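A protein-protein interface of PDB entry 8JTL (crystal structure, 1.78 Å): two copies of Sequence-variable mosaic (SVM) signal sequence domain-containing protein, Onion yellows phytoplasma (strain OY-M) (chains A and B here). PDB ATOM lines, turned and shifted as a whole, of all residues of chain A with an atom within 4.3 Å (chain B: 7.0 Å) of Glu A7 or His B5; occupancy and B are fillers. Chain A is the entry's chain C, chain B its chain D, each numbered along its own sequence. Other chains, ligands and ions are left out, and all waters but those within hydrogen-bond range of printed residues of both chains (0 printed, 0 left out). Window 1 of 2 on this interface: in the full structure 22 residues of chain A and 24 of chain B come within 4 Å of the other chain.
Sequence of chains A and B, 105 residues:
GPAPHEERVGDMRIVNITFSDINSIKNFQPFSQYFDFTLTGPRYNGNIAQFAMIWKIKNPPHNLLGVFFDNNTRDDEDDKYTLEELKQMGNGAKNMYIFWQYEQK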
ATOM      1  N   HIS A   5     -14.813   0.751   6.070  1.00  0.00           N
ATOM      2  CA  HIS A   5     -16.136   0.229   5.857  1.00  0.00           C
ATOM      3  C   HIS A   5     -17.195   1.280   6.176  1.00  0.00           C
ATOM      4  O   HIS A   5     -17.106   2.016   7.156  1.00  0.00           O
ATOM      5  CB  HIS A   5     -16.364  -0.993   6.724  1.00  0.00           C
ATOM      6  CG  HIS A   5     -17.733  -1.539   6.580  1.00  0.00           C
ATOM      7  ND1 HIS A   5     -18.799  -1.098   7.338  1.00  0.00           N
ATOM      8  CD2 HIS A   5     -18.228  -2.440   5.699  1.00  0.00           C
ATOM      9  CE1 HIS A   5     -19.894  -1.724   6.929  1.00  0.00           C
ATOM     10  NE2 HIS A   5     -19.565  -2.559   5.954  1.00  0.00           N
ATOM     11  N   GLU A   6     -18.251   1.292   5.382  1.00  0.00           N
ATOM     12  CA  GLU A   6     -19.318   2.228   5.642  1.00  0.00           C
ATOM     13  C   GLU A   6     -20.604   1.549   5.238  1.00  0.00           C
ATOM     14  O   GLU A   6     -20.699   1.004   4.145  1.00  0.00           O
ATOM     15  CB  GLU A   6     -19.138   3.501   4.835  1.00  0.00           C
ATOM     16  CG  GLU A   6     -20.352   4.391   4.934  1.00  0.00           C
ATOM     17  CD  GLU A   6     -20.074   5.775   4.424  1.00  0.00           C
ATOM     18  OE1 GLU A   6     -19.392   5.879   3.382  1.00  0.00           O
ATOM     19  OE2 GLU A   6     -20.532   6.740   5.073  1.00  0.00           O
ATOM     20  N   GLU A   7     -21.571   1.539   6.126  1.00  0.00           N
ATOM     21  CA  GLU A   7     -22.919   1.207   5.718  1.00  0.00           C
ATOM     22  C   GLU A   7     -23.789   2.386   6.118  1.00  0.00           C
ATOM     23  O   GLU A   7     -23.666   2.915   7.238  1.00  0.00           O
ATOM     24  CB  GLU A   7     -23.416  -0.092   6.341  1.00  0.00           C
ATOM     25  CG  GLU A   7     -24.751  -0.482   5.713  1.00  0.00           C
ATOM     26  CD  GLU A   7     -25.289  -1.779   6.239  1.00  0.00           C
ATOM     27  OE1 GLU A   7     -24.607  -2.457   7.059  1.00  0.00           O
ATOM     28  OE2 GLU A   7     -26.423  -2.087   5.856  1.00  0.00           O
ATOM     29  N   ARG A   8     -24.643   2.821   5.216  1.00  0.00           N
ATOM     30  CA  ARG A   8     -25.483   3.940   5.604  1.00  0.00           C
ATOM     31  C   ARG A   8     -26.753   3.927   4.793  1.00  0.00           C
ATOM     32  O   ARG A   8     -26.834   3.287   3.748  1.00  0.00           O
ATOM     33  CB  ARG A   8     -24.792   5.295   5.443  1.00  0.00           C
ATOM     34  CG  ARG A   8     -24.550   5.826   4.030  1.00  0.00           C
ATOM     35  CD  ARG A   8     -23.775   7.178   4.113  1.00  0.00           C
ATOM     36  NE  ARG A   8     -22.913   7.274   5.295  1.00  0.00           N
ATOM     37  CZ  ARG A   8     -23.108   8.052   6.360  1.00  0.00           C
ATOM     38  NH1 ARG A   8     -24.157   8.858   6.463  1.00  0.00           N
ATOM     39  NH2 ARG A   8     -22.242   7.994   7.368  1.00  0.00           N
ATOM     40  N   VAL A   9     -27.748   4.647   5.315  1.00  0.00           N
ATOM     41  CA  VAL A   9     -28.934   5.005   4.552  1.00  0.00           C
ATOM     42  C   VAL A   9     -29.048   6.507   4.678  1.00  0.00           C
ATOM     43  O   VAL A   9     -29.332   7.016   5.769  1.00  0.00           O
ATOM     44  CB  VAL A   9     -30.201   4.307   5.057  1.00  0.00           C
ATOM     45  CG1 VAL A   9     -31.423   4.892   4.348  1.00  0.00           C
ATOM     46  CG2 VAL A   9     -30.085   2.750   4.828  1.00  0.00           C
ATOM     47  N   ARG A  13     -25.889   6.616   9.599  1.00  0.00           N
ATOM     48  CA  ARG A  13     -24.863   5.594   9.637  1.00  0.00           C
ATOM     49  C   ARG A  13     -25.457   4.293  10.148  1.00  0.00           C
ATOM     50  O   ARG A  13     -26.261   4.285  11.083  1.00  0.00           O
ATOM     51  CB  ARG A  13     -23.737   6.051  10.543  1.00  0.00           C
ATOM     52  CG  ARG A  13     -22.556   5.100  10.549  1.00  0.00           C
ATOM     53  CD  ARG A  13     -21.483   5.568  11.499  1.00  0.00           C
ATOM     54  NE  ARG A  13     -20.887   6.836  11.077  1.00  0.00           N
ATOM     55  CZ  ARG A  13     -21.062   7.987  11.702  1.00  0.00           C
ATOM     56  NH1 ARG A  13     -21.889   8.092  12.750  1.00  0.00           N
ATOM     57  NH2 ARG A  13     -20.389   9.066  11.275  1.00  0.00           N
ATOM     58  N   ILE A  14     -25.079   3.188   9.528  1.00  0.00           N
ATOM     59  CA  ILE A  14     -25.515   1.893   9.991  1.00  0.00           C
ATOM     60  C   ILE A  14     -24.307   1.258  10.633  1.00  0.00           C
ATOM     61  O   ILE A  14     -23.248   1.125  10.009  1.00  0.00           O
ATOM     62  CB  ILE A  14     -26.108   1.031   8.871  1.00  0.00           C
ATOM     63  CG1 ILE A  14     -27.405   1.704   8.404  1.00  0.00           C
ATOM     64  CG2 ILE A  14     -26.287  -0.405   9.379  1.00  0.00           C
ATOM     65  CD1 ILE A  14     -28.133   1.002   7.305  1.00  0.00           C
ATOM     66  N   ASN A  16     -22.817  -1.758  12.461  1.00  0.00           N
ATOM     67  CA  ASN A  16     -22.922  -3.184  12.711  1.00  0.00           C
ATOM     68  C   ASN A  16     -21.986  -3.545  13.839  1.00  0.00           C
ATOM     69  O   ASN A  16     -20.774  -3.348  13.732  1.00  0.00           O
ATOM     70  CB  ASN A  16     -22.584  -4.005  11.474  1.00  0.00           C
ATOM     71  CG  ASN A  16     -23.578  -3.768  10.384  1.00  0.00           C
ATOM     72  OD1 ASN A  16     -24.684  -4.298  10.428  1.00  0.00           O
ATOM     73  ND2 ASN A  16     -23.232  -2.905   9.444  1.00  0.00           N
ATOM     74  N   LYS A  87     -33.810  -0.303   7.845  1.00  0.00           N
ATOM     75  CA  LYS A  87     -32.746   0.601   7.464  1.00  0.00           C
ATOM     76  C   LYS A  87     -33.304   1.870   6.851  1.00  0.00           C
ATOM     77  O   LYS A  87     -32.642   2.906   6.835  1.00  0.00           O
ATOM     78  CB  LYS A  87     -31.789  -0.120   6.516  1.00  0.00           C
ATOM     79  CG  LYS A  87     -31.155  -1.365   7.150  1.00  0.00           C
ATOM     80  CD  LYS A  87     -30.144  -2.008   6.210  1.00  0.00           C
ATOM     81  CE  LYS A  87     -29.455  -3.194   6.885  1.00  0.00           C
ATOM     82  NZ  LYS A  87     -28.490  -3.855   5.971  1.00  0.00           N
ATOM     83  N   ALA B   3     -33.966   6.630   1.614  1.00  0.00           N
ATOM     84  CA  ALA B   3     -32.738   7.140   1.037  1.00  0.00           C
ATOM     85  C   ALA B   3     -31.997   5.945   0.468  1.00  0.00           C
ATOM     86  O   ALA B   3     -32.298   4.806   0.829  1.00  0.00           O
ATOM     87  CB  ALA B   3     -31.899   7.887   2.078  1.00  0.00           C
ATOM     88  N   PRO B   4     -31.030   6.168  -0.420  1.00  0.00           N
ATOM     89  CA  PRO B   4     -30.246   5.044  -0.936  1.00  0.00           C
ATOM     90  C   PRO B   4     -29.522   4.343   0.201  1.00  0.00           C
ATOM     91  O   PRO B   4     -28.892   4.973   1.044  1.00  0.00           O
ATOM     92  CB  PRO B   4     -29.255   5.711  -1.903  1.00  0.00           C
ATOM     93  CG  PRO B   4     -29.917   7.036  -2.255  1.00  0.00           C
ATOM     94  CD  PRO B   4     -30.579   7.454  -0.982  1.00  0.00           C
ATOM     95  N   HIS B   5     -29.600   3.029   0.205  1.00  0.00           N
ATOM     96  CA  HIS B   5     -28.752   2.259   1.085  1.00  0.00           C
ATOM     97  C   HIS B   5     -27.405   2.093   0.412  1.00  0.00           C
ATOM     98  O   HIS B   5     -27.338   1.845  -0.790  1.00  0.00           O
ATOM     99  CB  HIS B   5     -29.353   0.890   1.354  1.00  0.00           C
ATOM    100  CG  HIS B   5     -28.425  -0.006   2.093  1.00  0.00           C
ATOM    101  ND1 HIS B   5     -27.536  -0.843   1.458  1.00  0.00           N
ATOM    102  CD2 HIS B   5     -28.181  -0.134   3.424  1.00  0.00           C
ATOM    103  CE1 HIS B   5     -26.813  -1.479   2.362  1.00  0.00           C
ATOM    104  NE2 HIS B   5     -27.182  -1.067   3.562  1.00  0.00           N
ATOM    105  N   GLU B   6     -26.329   2.281   1.158  1.00  0.00           N
ATOM    106  CA  GLU B   6     -25.054   1.903   0.579  1.00  0.00           C
ATOM    107  C   GLU B   6     -24.217   1.201   1.623  1.00  0.00           C
ATOM    108  O   GLU B   6     -24.172   1.589   2.785  1.00  0.00           O
ATOM    109  CB  GLU B   6     -24.228   3.068  -0.021  1.00  0.00           C
ATOM    110  CG  GLU B   6     -23.557   3.978   0.944  1.00  0.00           C
ATOM    111  CD  GLU B   6     -22.596   4.967   0.252  1.00  0.00           C
ATOM    112  OE1 GLU B   6     -22.386   4.852  -0.977  1.00  0.00           O
ATOM    113  OE2 GLU B   6     -22.024   5.840   0.955  1.00  0.00           O
ATOM    114  N   GLU B   7     -23.588   0.140   1.203  1.00  0.00           N
ATOM    115  CA  GLU B   7     -22.555  -0.467   2.004  1.00  0.00           C
ATOM    116  C   GLU B   7     -21.332  -0.503   1.120  1.00  0.00           C
ATOM    117  O   GLU B   7     -21.429  -0.838  -0.061  1.00  0.00           O
ATOM    118  CB  GLU B   7     -22.911  -1.873   2.478  1.00  0.00           C
ATOM    119  CG  GLU B   7     -21.865  -2.316   3.475  1.00  0.00           C
ATOM    120  CD  GLU B   7     -22.042  -3.698   3.989  1.00  0.00           C
ATOM    121  OE1 GLU B   7     -23.066  -4.313   3.636  1.00  0.00           O
ATOM    122  OE2 GLU B   7     -21.136  -4.172   4.731  1.00  0.00           O
ATOM    123  N   ARG B   8     -20.188  -0.141   1.680  1.00  0.00           N
ATOM    124  CA  ARG B   8     -19.011  -0.129   0.846  1.00  0.00           C
ATOM    125  C   ARG B   8     -17.776  -0.217   1.720  1.00  0.00           C
ATOM    126  O   ARG B   8     -17.793   0.100   2.917  1.00  0.00           O
ATOM    127  CB  ARG B   8     -18.983   1.111  -0.067  1.00  0.00           C
ATOM    128  CG  ARG B   8     -18.657   2.472   0.553  1.00  0.00           C
ATOM    129  CD  ARG B   8     -18.629   3.478  -0.631  1.00  0.00           C
ATOM    130  NE  ARG B   8     -19.530   3.049  -1.713  1.00  0.00           N
ATOM    131  CZ  ARG B   8     -19.220   2.927  -3.006  1.00  0.00           C
ATOM    132  NH1 ARG B   8     -17.992   3.139  -3.456  1.00  0.00           N
ATOM    133  NH2 ARG B   8     -20.149   2.517  -3.860  1.00  0.00           N
ATOM    134  N   ILE B  14     -20.549  -2.915  -1.591  1.00  0.00           N
ATOM    135  CA  ILE B  14     -20.965  -4.165  -1.013  1.00  0.00           C
ATOM    136  C   ILE B  14     -22.432  -4.329  -1.305  1.00  0.00           C
ATOM    137  O   ILE B  14     -23.248  -3.463  -0.986  1.00  0.00           O
ATOM    138  CB  ILE B  14     -20.671  -4.208   0.488  1.00  0.00           C
ATOM    139  CG1 ILE B  14     -19.142  -4.157   0.637  1.00  0.00           C
ATOM    140  CG2 ILE B  14     -21.312  -5.432   1.104  1.00  0.00           C
ATOM    141  CD1 ILE B  14     -18.693  -4.038   2.080  1.00  0.00           C
ATOM    142  N   VAL B  15     -22.760  -5.413  -1.986  1.00  0.00           N
ATOM    143  CA  VAL B  15     -24.079  -5.593  -2.537  1.00  0.00           C
ATOM    144  C   VAL B  15     -24.652  -6.794  -1.845  1.00  0.00           C
ATOM    145  O   VAL B  15     -24.214  -7.932  -2.080  1.00  0.00           O
ATOM    146  CB  VAL B  15     -24.048  -5.796  -4.051  1.00  0.00           C
ATOM    147  CG1 VAL B  15     -25.456  -5.841  -4.602  1.00  0.00           C
ATOM    148  CG2 VAL B  15     -23.246  -4.674  -4.704  1.00  0.00           C
ATOM    149  N   ASN B  16     -25.592  -6.545  -0.964  1.00  0.00           N
ATOM    150  CA  ASN B  16     -26.220  -7.600  -0.207  1.00  0.00           C
ATOM    151  C   ASN B  16     -27.428  -8.056  -0.993  1.00  0.00           C
ATOM    152  O   ASN B  16     -28.262  -7.255  -1.397  1.00  0.00           O
ATOM    153  CB  ASN B  16     -26.627  -7.093   1.163  1.00  0.00           C
ATOM    154  CG  ASN B  16     -25.436  -6.726   1.976  1.00  0.00           C
ATOM    155  OD1 ASN B  16     -24.801  -7.582   2.539  1.00  0.00           O
ATOM    156  ND2 ASN B  16     -25.086  -5.434   1.982  1.00  0.00           N
ATOM    157  N   LYS B  87     -14.644  -8.304   3.631  1.00  0.00           N
ATOM    158  CA  LYS B  87     -14.967  -6.966   3.148  1.00  0.00           C
ATOM    159  C   LYS B  87     -13.730  -6.121   2.913  1.00  0.00           C
ATOM    160  O   LYS B  87     -13.830  -5.105   2.224  1.00  0.00           O
ATOM    161  CB  LYS B  87     -15.909  -6.261   4.121  1.00  0.00           C
ATOM    162  CG  LYS B  87     -17.209  -7.005   4.321  1.00  0.00           C
ATOM    163  CD  LYS B  87     -18.227  -6.205   5.170  1.00  0.00           C
ATOM    164  CE  LYS B  87     -19.451  -7.085   5.475  1.00  0.00           C
ATOM    165  NZ  LYS B  87     -20.536  -6.380   6.209  1.00  0.00           N
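The side-chain carboxylate (OE2) of Glu A7 is in hydrogen-bond range of a ring nitrogen (NE2) of His B5 (2.6 Å). The backbone NH of Arg A8 lies within hydrogen-bond range of the backbone carbonyl oxygen of Glu B6 (2.8 Å). The side-chain carboxylate (OE2) of Glu B7 lies within hydrogen-bond range of a ring nitrogen (NE2) of His A5 (2.6 Å). The backbone NH (N) of Arg B8 sits at hydrogen-bond distance from the backbone carbonyl oxygen (O) of Glu A6 (2.8 Å).
OE1 of Glu B6 is in salt-bridge range of NE of Arg B8 (3.5 Å). The side-chain amide nitrogen (ND2) of Asn B16 sits at hydrogen-bond distance from the side-chain carboxylate (OE1) of Glu B7 (2.8 Å). OE2 of Glu B7 lies within salt-bridge range of NZ of Lys B87, at 2.7 Å. OE2 of Glu A6 is in salt-bridge range of NE of Arg A8, at 2.5 Å. The backbone NH of Ile A14 is in hydrogen-bond range of the backbone carbonyl oxygen of Glu A7. OE1 of Glu A7 is in hydrogen-bond range of ND2 of Asn A16, at 2.8 Å.
Among the printed residues, pairs that only touch across the chains: His A5 with Arg B8, His A5 with Ile B14, His A5 with Lys B87, Glu A6 with Glu B6, Glu A6 with Glu B7, Glu A7 with Glu B6, Glu A7 with Glu B7, Arg A8 with Pro B4, Arg A8 with His B5, Val A9 with Ala B3, Val A9 with Pro B4, Val A9 with His B5 and Lys A87 with His B5.
Glu A7 touches just these residues of chain B: His B5 (2.6 Å), Glu B6 (3.2 Å) and Glu B7 (3.9 Å). Of chain A, only Glu A7, Arg A8, Val A9 and Lys A87 come within 4 Å of His B5. Printed residues of chain B within 4 Å of Val A9: Ala B3, Pro B4 and His B5. Of the printed residues of chain A, Pro B4 touches Arg A8 and Val A9. Of the printed residues of chain A, Glu B6 touches Glu A6 (3.6 Å), Glu A7 (3.2 Å) and Arg A8 (2.8 Å). The nearest residue of chain B that does not touch Glu A7 is Arg B8 (4.9 Å). The nearest residue of chain A that does not touch His B5 is Ile A14 (4.04 Å).
Printed residues of chain A that touch a printed residue of chain B: His A5, Glu A6, Glu A7, Arg A8, Val A9 and Lys A87. Of the 10 printed residues of chain B, 8 touch a printed residue of chain A. Among the printed residues, 17 pairs touch across the chains. Among the printed residues, no Asp or Glu carboxylate lies within 4 Å of a Lys or Arg side-chain nitrogen of the other chain.
His A5 touches Glu B7, and with the chains exchanged Glu A7 touches His B5. His A5 touches Arg B8, and with the chains exchanged Arg A8 touches His B5. Glu A6 touches Glu B7, and with the chains exchanged Glu A7 touches Glu B6. Glu B7 touches its own counterpart, Glu A7. Positions printed for both chains: 5, 6, 7, 8, 14, 16 and 87.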
